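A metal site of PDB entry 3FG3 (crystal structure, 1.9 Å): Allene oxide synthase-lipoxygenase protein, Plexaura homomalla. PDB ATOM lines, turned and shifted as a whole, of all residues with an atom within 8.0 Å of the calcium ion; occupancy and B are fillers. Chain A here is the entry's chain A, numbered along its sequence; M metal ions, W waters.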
ATOM      1  N   THR A  15      22.568  10.931   6.613  1.00  0.00           N
ATOM      2  CA  THR A  15      22.891  11.464   7.950  1.00  0.00           C
ATOM      3  C   THR A  15      22.091  12.810   8.166  1.00  0.00           C
ATOM      4  O   THR A  15      21.978  13.637   7.242  1.00  0.00           O
ATOM      5  CB  THR A  15      24.405  11.666   8.090  1.00  0.00           C
ATOM      6  OG1 THR A  15      25.087  10.382   8.002  1.00  0.00           O
ATOM      7  CG2 THR A  15      24.816  12.372   9.402  1.00  0.00           C
ATOM      8  N   ARG A  18      21.554  18.063  11.457  1.00  0.00           N
ATOM      9  CA  ARG A  18      21.798  18.805  12.682  1.00  0.00           C
ATOM     10  C   ARG A  18      23.284  18.773  13.136  1.00  0.00           C
ATOM     11  O   ARG A  18      24.044  17.844  12.811  1.00  0.00           O
ATOM     12  CB  ARG A  18      20.872  18.360  13.818  1.00  0.00           C
ATOM     13  CG  ARG A  18      21.211  16.870  14.399  1.00  0.00           C
ATOM     14  CD  ARG A  18      19.992  16.283  15.166  1.00  0.00           C
ATOM     15  NE  ARG A  18      18.784  16.168  14.278  1.00  0.00           N
ATOM     16  CZ  ARG A  18      17.548  15.899  14.744  1.00  0.00           C
ATOM     17  NH1 ARG A  18      17.393  15.786  16.077  1.00  0.00           N
ATOM     18  NH2 ARG A  18      16.489  15.736  13.875  1.00  0.00           N
ATOM     19  N   GLU A  19      23.688  19.831  13.838  1.00  0.00           N
ATOM     20  CA  GLU A  19      25.048  19.908  14.338  1.00  0.00           C
ATOM     21  C   GLU A  19      25.461  18.614  15.077  1.00  0.00           C
ATOM     22  O   GLU A  19      24.691  18.098  15.886  1.00  0.00           O
ATOM     23  CB  GLU A  19      25.215  21.107  15.295  1.00  0.00           C
ATOM     24  CG  GLU A  19      25.433  22.405  14.470  1.00  0.00           C
ATOM     25  CD  GLU A  19      25.217  23.641  15.336  1.00  0.00           C
ATOM     26  OE1 GLU A  19      24.763  24.686  14.791  1.00  0.00           O
ATOM     27  OE2 GLU A  19      25.460  23.489  16.554  1.00  0.00           O
ATOM     28  N   HIS A  20      26.665  18.130  14.752  1.00  0.00           N
ATOM     29  CA  HIS A  20      27.284  16.922  15.411  1.00  0.00           C
ATOM     30  C   HIS A  20      26.620  15.654  14.937  1.00  0.00           C
ATOM     31  O   HIS A  20      26.987  14.599  15.386  1.00  0.00           O
ATOM     32  CB  HIS A  20      27.308  16.999  16.926  1.00  0.00           C
ATOM     33  CG  HIS A  20      28.238  18.050  17.429  1.00  0.00           C
ATOM     34  ND1 HIS A  20      29.485  18.238  16.874  1.00  0.00           N
ATOM     35  CD2 HIS A  20      28.104  18.977  18.391  1.00  0.00           C
ATOM     36  CE1 HIS A  20      30.091  19.247  17.484  1.00  0.00           C
ATOM     37  NE2 HIS A  20      29.280  19.700  18.426  1.00  0.00           N
ATOM     38  N   ALA A  21      25.750  15.759  13.949  1.00  0.00           N
ATOM     39  CA  ALA A  21      25.094  14.552  13.410  1.00  0.00           C
ATOM     40  C   ALA A  21      26.132  13.542  12.839  1.00  0.00           C
ATOM     41  O   ALA A  21      25.903  12.322  12.818  1.00  0.00           O
ATOM     42  CB  ALA A  21      24.150  14.946  12.325  1.00  0.00           C
ATOM     43  N   GLY A  22      27.212  14.097  12.300  1.00  0.00           N
ATOM     44  CA  GLY A  22      28.226  13.304  11.569  1.00  0.00           C
ATOM     45  C   GLY A  22      29.042  12.418  12.470  1.00  0.00           C
ATOM     46  O   GLY A  22      28.958  12.497  13.729  1.00  0.00           O
ATOM     47  N   THR A  23      29.901  11.574  11.869  1.00  0.00           N
ATOM     48  CA  THR A  23      30.724  10.744  12.745  1.00  0.00           C
ATOM     49  C   THR A  23      31.982  10.375  11.968  1.00  0.00           C
ATOM     50  O   THR A  23      31.932  10.282  10.722  1.00  0.00           O
ATOM     51  CB  THR A  23      29.998   9.440  13.198  1.00  0.00           C
ATOM     52  OG1 THR A  23      30.834   8.740  14.106  1.00  0.00           O
ATOM     53  CG2 THR A  23      29.665   8.532  12.028  1.00  0.00           C
ATOM     54  N   ASP A  24      33.066  10.134  12.694  1.00  0.00           N
ATOM     55  CA  ASP A  24      34.206   9.400  12.131  1.00  0.00           C
ATOM     56  C   ASP A  24      34.479   8.042  12.745  1.00  0.00           C
ATOM     57  O   ASP A  24      35.540   7.448  12.512  1.00  0.00           O
ATOM     58  CB  ASP A  24      35.446  10.288  12.125  1.00  0.00           C
ATOM     59  CG  ASP A  24      36.002  10.532  13.520  1.00  0.00           C
ATOM     60  OD1 ASP A  24      35.495  10.028  14.529  1.00  0.00           O
ATOM     61  OD2 ASP A  24      36.997  11.290  13.603  1.00  0.00           O
ATOM     62  N   ALA A  25      33.510   7.511  13.477  1.00  0.00           N
ATOM     63  CA  ALA A  25      33.625   6.145  13.956  1.00  0.00           C
ATOM     64  C   ALA A  25      33.647   5.214  12.758  1.00  0.00           C
ATOM     65  O   ALA A  25      33.177   5.579  11.667  1.00  0.00           O
ATOM     66  CB  ALA A  25      32.440   5.801  14.865  1.00  0.00           C
ATOM     67  N   PHE A  48      31.062  10.502   6.772  1.00  0.00           N
ATOM     68  CA  PHE A  48      29.706  10.734   7.188  1.00  0.00           C
ATOM     69  C   PHE A  48      29.568  12.132   7.798  1.00  0.00           C
ATOM     70  O   PHE A  48      29.605  12.288   9.032  1.00  0.00           O
ATOM     71  CB  PHE A  48      29.341   9.665   8.227  1.00  0.00           C
ATOM     72  CG  PHE A  48      29.056   8.292   7.625  1.00  0.00           C
ATOM     73  CD1 PHE A  48      29.727   7.184   8.076  1.00  0.00           C
ATOM     74  CD2 PHE A  48      28.102   8.143   6.615  1.00  0.00           C
ATOM     75  CE1 PHE A  48      29.437   5.919   7.520  1.00  0.00           C
ATOM     76  CE2 PHE A  48      27.796   6.901   6.100  1.00  0.00           C
ATOM     77  CZ  PHE A  48      28.480   5.788   6.581  1.00  0.00           C
ATOM     78  N   ALA A  50      27.398  15.728   8.516  1.00  0.00           N
ATOM     79  CA  ALA A  50      25.933  16.140   8.686  1.00  0.00           C
ATOM     80  C   ALA A  50      25.306  16.454   7.330  1.00  0.00           C
ATOM     81  O   ALA A  50      25.967  17.109   6.469  1.00  0.00           O
ATOM     82  CB  ALA A  50      25.846  17.339   9.665  1.00  0.00           C
ATOM     83  N   GLY A  81      36.153  13.442  18.095  1.00  0.00           N
ATOM     84  CA  GLY A  81      35.571  14.437  18.976  1.00  0.00           C
ATOM     85  C   GLY A  81      34.126  14.081  19.371  1.00  0.00           C
ATOM     86  O   GLY A  81      33.779  14.163  20.562  1.00  0.00           O
ATOM     87  N   ASP A  82      33.283  13.678  18.389  1.00  0.00           N
ATOM     88  CA  ASP A  82      31.864  13.313  18.719  1.00  0.00           C
ATOM     89  C   ASP A  82      31.351  12.127  17.849  1.00  0.00           C
ATOM     90  O   ASP A  82      30.637  12.313  16.871  1.00  0.00           O
ATOM     91  CB  ASP A  82      30.968  14.571  18.682  1.00  0.00           C
ATOM     92  CG  ASP A  82      29.523  14.258  19.085  1.00  0.00           C
ATOM     93  OD1 ASP A  82      29.244  14.159  20.285  1.00  0.00           O
ATOM     94  OD2 ASP A  82      28.676  14.050  18.183  1.00  0.00           O
ATOM     95  N   PRO A  83      31.768  10.885  18.199  1.00  0.00           N
ATOM     96  CA  PRO A  83      31.423   9.657  17.456  1.00  0.00           C
ATOM     97  C   PRO A  83      29.916   9.405  17.307  1.00  0.00           C
ATOM     98  O   PRO A  83      29.478   8.811  16.288  1.00  0.00           O
ATOM     99  CB  PRO A  83      32.118   8.532  18.250  1.00  0.00           C
ATOM    100  CG  PRO A  83      32.383   9.113  19.644  1.00  0.00           C
ATOM    101  CD  PRO A  83      32.614  10.610  19.374  1.00  0.00           C
ATOM    102  N   ASP A  84      29.078   9.920  18.229  1.00  0.00           N
ATOM    103  CA  ASP A  84      27.632   9.672  18.100  1.00  0.00           C
ATOM    104  C   ASP A  84      27.151  10.207  16.737  1.00  0.00           C
ATOM    105  O   ASP A  84      27.584  11.237  16.258  1.00  0.00           O
ATOM    106  CB  ASP A  84      26.803  10.309  19.196  1.00  0.00           C
ATOM    107  CG  ASP A  84      27.090   9.764  20.592  1.00  0.00           C
ATOM    108  OD1 ASP A  84      26.611  10.449  21.525  1.00  0.00           O
ATOM    109  OD2 ASP A  84      27.712   8.667  20.757  1.00  0.00           O
ATOM    110  N   TRP A  85      26.207   9.512  16.134  1.00  0.00           N
ATOM    111  CA  TRP A  85      25.894   9.672  14.724  1.00  0.00           C
ATOM    112  C   TRP A  85      24.375   9.752  14.557  1.00  0.00           C
ATOM    113  O   TRP A  85      23.682   8.784  14.883  1.00  0.00           O
ATOM    114  CB  TRP A  85      26.416   8.445  13.969  1.00  0.00           C
ATOM    115  CG  TRP A  85      26.215   8.366  12.473  1.00  0.00           C
ATOM    116  CD1 TRP A  85      26.165   9.410  11.556  1.00  0.00           C
ATOM    117  CD2 TRP A  85      26.143   7.160  11.694  1.00  0.00           C
ATOM    118  NE1 TRP A  85      26.010   8.924  10.250  1.00  0.00           N
ATOM    119  CE2 TRP A  85      26.011   7.545  10.312  1.00  0.00           C
ATOM    120  CE3 TRP A  85      26.180   5.802  12.012  1.00  0.00           C
ATOM    121  CZ2 TRP A  85      25.918   6.601   9.276  1.00  0.00           C
ATOM    122  CZ3 TRP A  85      26.028   4.846  10.927  1.00  0.00           C
ATOM    123  CH2 TRP A  85      25.903   5.276   9.602  1.00  0.00           C
ATOM    124  N   PHE A  86      23.844  10.873  14.051  1.00  0.00           N
ATOM    125  CA  PHE A  86      22.411  10.957  13.880  1.00  0.00           C
ATOM    126  C   PHE A  86      22.009  10.495  12.481  1.00  0.00           C
ATOM    127  O   PHE A  86      22.296  11.172  11.499  1.00  0.00           O
ATOM    128  CB  PHE A  86      21.893  12.400  14.134  1.00  0.00           C
ATOM    129  CG  PHE A  86      20.396  12.473  14.218  1.00  0.00           C
ATOM    130  CD1 PHE A  86      19.749  12.397  15.458  1.00  0.00           C
ATOM    131  CD2 PHE A  86      19.616  12.504  13.067  1.00  0.00           C
ATOM    132  CE1 PHE A  86      18.336  12.430  15.520  1.00  0.00           C
ATOM    133  CE2 PHE A  86      18.196  12.573  13.138  1.00  0.00           C
ATOM    134  CZ  PHE A  86      17.555  12.510  14.336  1.00  0.00           C
ATOM    135  N   TRP A 108      19.718   8.896  17.408  1.00  0.00           N
ATOM    136  CA  TRP A 108      21.172   8.859  17.503  1.00  0.00           C
ATOM    137  C   TRP A 108      21.681   7.415  17.534  1.00  0.00           C
ATOM    138  O   TRP A 108      21.154   6.606  18.290  1.00  0.00           O
ATOM    139  CB  TRP A 108      21.624   9.615  18.773  1.00  0.00           C
ATOM    140  CG  TRP A 108      21.456  11.050  18.594  1.00  0.00           C
ATOM    141  CD1 TRP A 108      20.349  11.847  18.945  1.00  0.00           C
ATOM    142  CD2 TRP A 108      22.411  11.950  18.015  1.00  0.00           C
ATOM    143  NE1 TRP A 108      20.588  13.169  18.593  1.00  0.00           N
ATOM    144  CE2 TRP A 108      21.866  13.268  18.069  1.00  0.00           C
ATOM    145  CE3 TRP A 108      23.708  11.758  17.474  1.00  0.00           C
ATOM    146  CZ2 TRP A 108      22.551  14.388  17.532  1.00  0.00           C
ATOM    147  CZ3 TRP A 108      24.422  12.889  16.983  1.00  0.00           C
ATOM    148  CH2 TRP A 108      23.834  14.167  16.985  1.00  0.00           C
ATOM    149  N   VAL A 109      22.745   7.142  16.783  1.00  0.00           N
ATOM    150  CA  VAL A 109      23.388   5.877  16.812  1.00  0.00           C
ATOM    151  C   VAL A 109      24.598   6.050  17.726  1.00  0.00           C
ATOM    152  O   VAL A 109      25.470   6.876  17.481  1.00  0.00           O
ATOM    153  CB  VAL A 109      23.813   5.385  15.409  1.00  0.00           C
ATOM    154  CG1 VAL A 109      24.696   4.089  15.531  1.00  0.00           C
ATOM    155  CG2 VAL A 109      22.528   5.187  14.508  1.00  0.00           C
ATOM    156  N   ARG A 169      20.654  10.936  24.514  1.00  0.00           N
ATOM    157  CA  ARG A 169      20.833  11.965  23.468  1.00  0.00           C
ATOM    158  C   ARG A 169      19.556  12.217  22.621  1.00  0.00           C
ATOM    159  O   ARG A 169      19.390  13.332  22.145  1.00  0.00           O
ATOM    160  CB  ARG A 169      22.046  11.637  22.564  1.00  0.00           C
ATOM    161  CG  ARG A 169      22.564  12.918  21.893  1.00  0.00           C
ATOM    162  CD  ARG A 169      23.981  12.730  21.433  1.00  0.00           C
ATOM    163  NE  ARG A 169      24.452  13.882  20.656  1.00  0.00           N
ATOM    164  CZ  ARG A 169      25.733  14.100  20.399  1.00  0.00           C
ATOM    165  NH1 ARG A 169      26.627  13.210  20.830  1.00  0.00           N
ATOM    166  NH2 ARG A 169      26.104  15.179  19.693  1.00  0.00           N
HETATM  167 CA    CA M   1      28.772  13.198  15.922  1.00  0.00          CA
HETATM  168  O   HOH W   1      30.130  14.936  15.175  1.00  0.00           O
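OD1 of Asp 82 lies within salt-bridge range of NH1 of Arg 169, at 2.8 Å. The side-chain carboxylate (OD1) of Asp 84 lies within salt-bridge range of the guanidinium group (NH1) of Arg 169, 2.8 Å away.
Within 4 Å of the calcium ion: His 20, Gly 22, Asp 82 and Asp 84.
O of Asp 82 binds the calcium ion. O of Gly 22 binds the calcium ion, at 2.3 Å. O of Asp 84 is bound to the calcium ion (2.3 Å). Water W1 binds the calcium ion (2.3 Å). The calcium ion is bound by O of His 20 (2.3 Å). The calcium ion is bound by the side-chain carboxylate (OD2) of Asp 82 (2.4 Å). The calcium ion has six donor atoms within binding distance.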
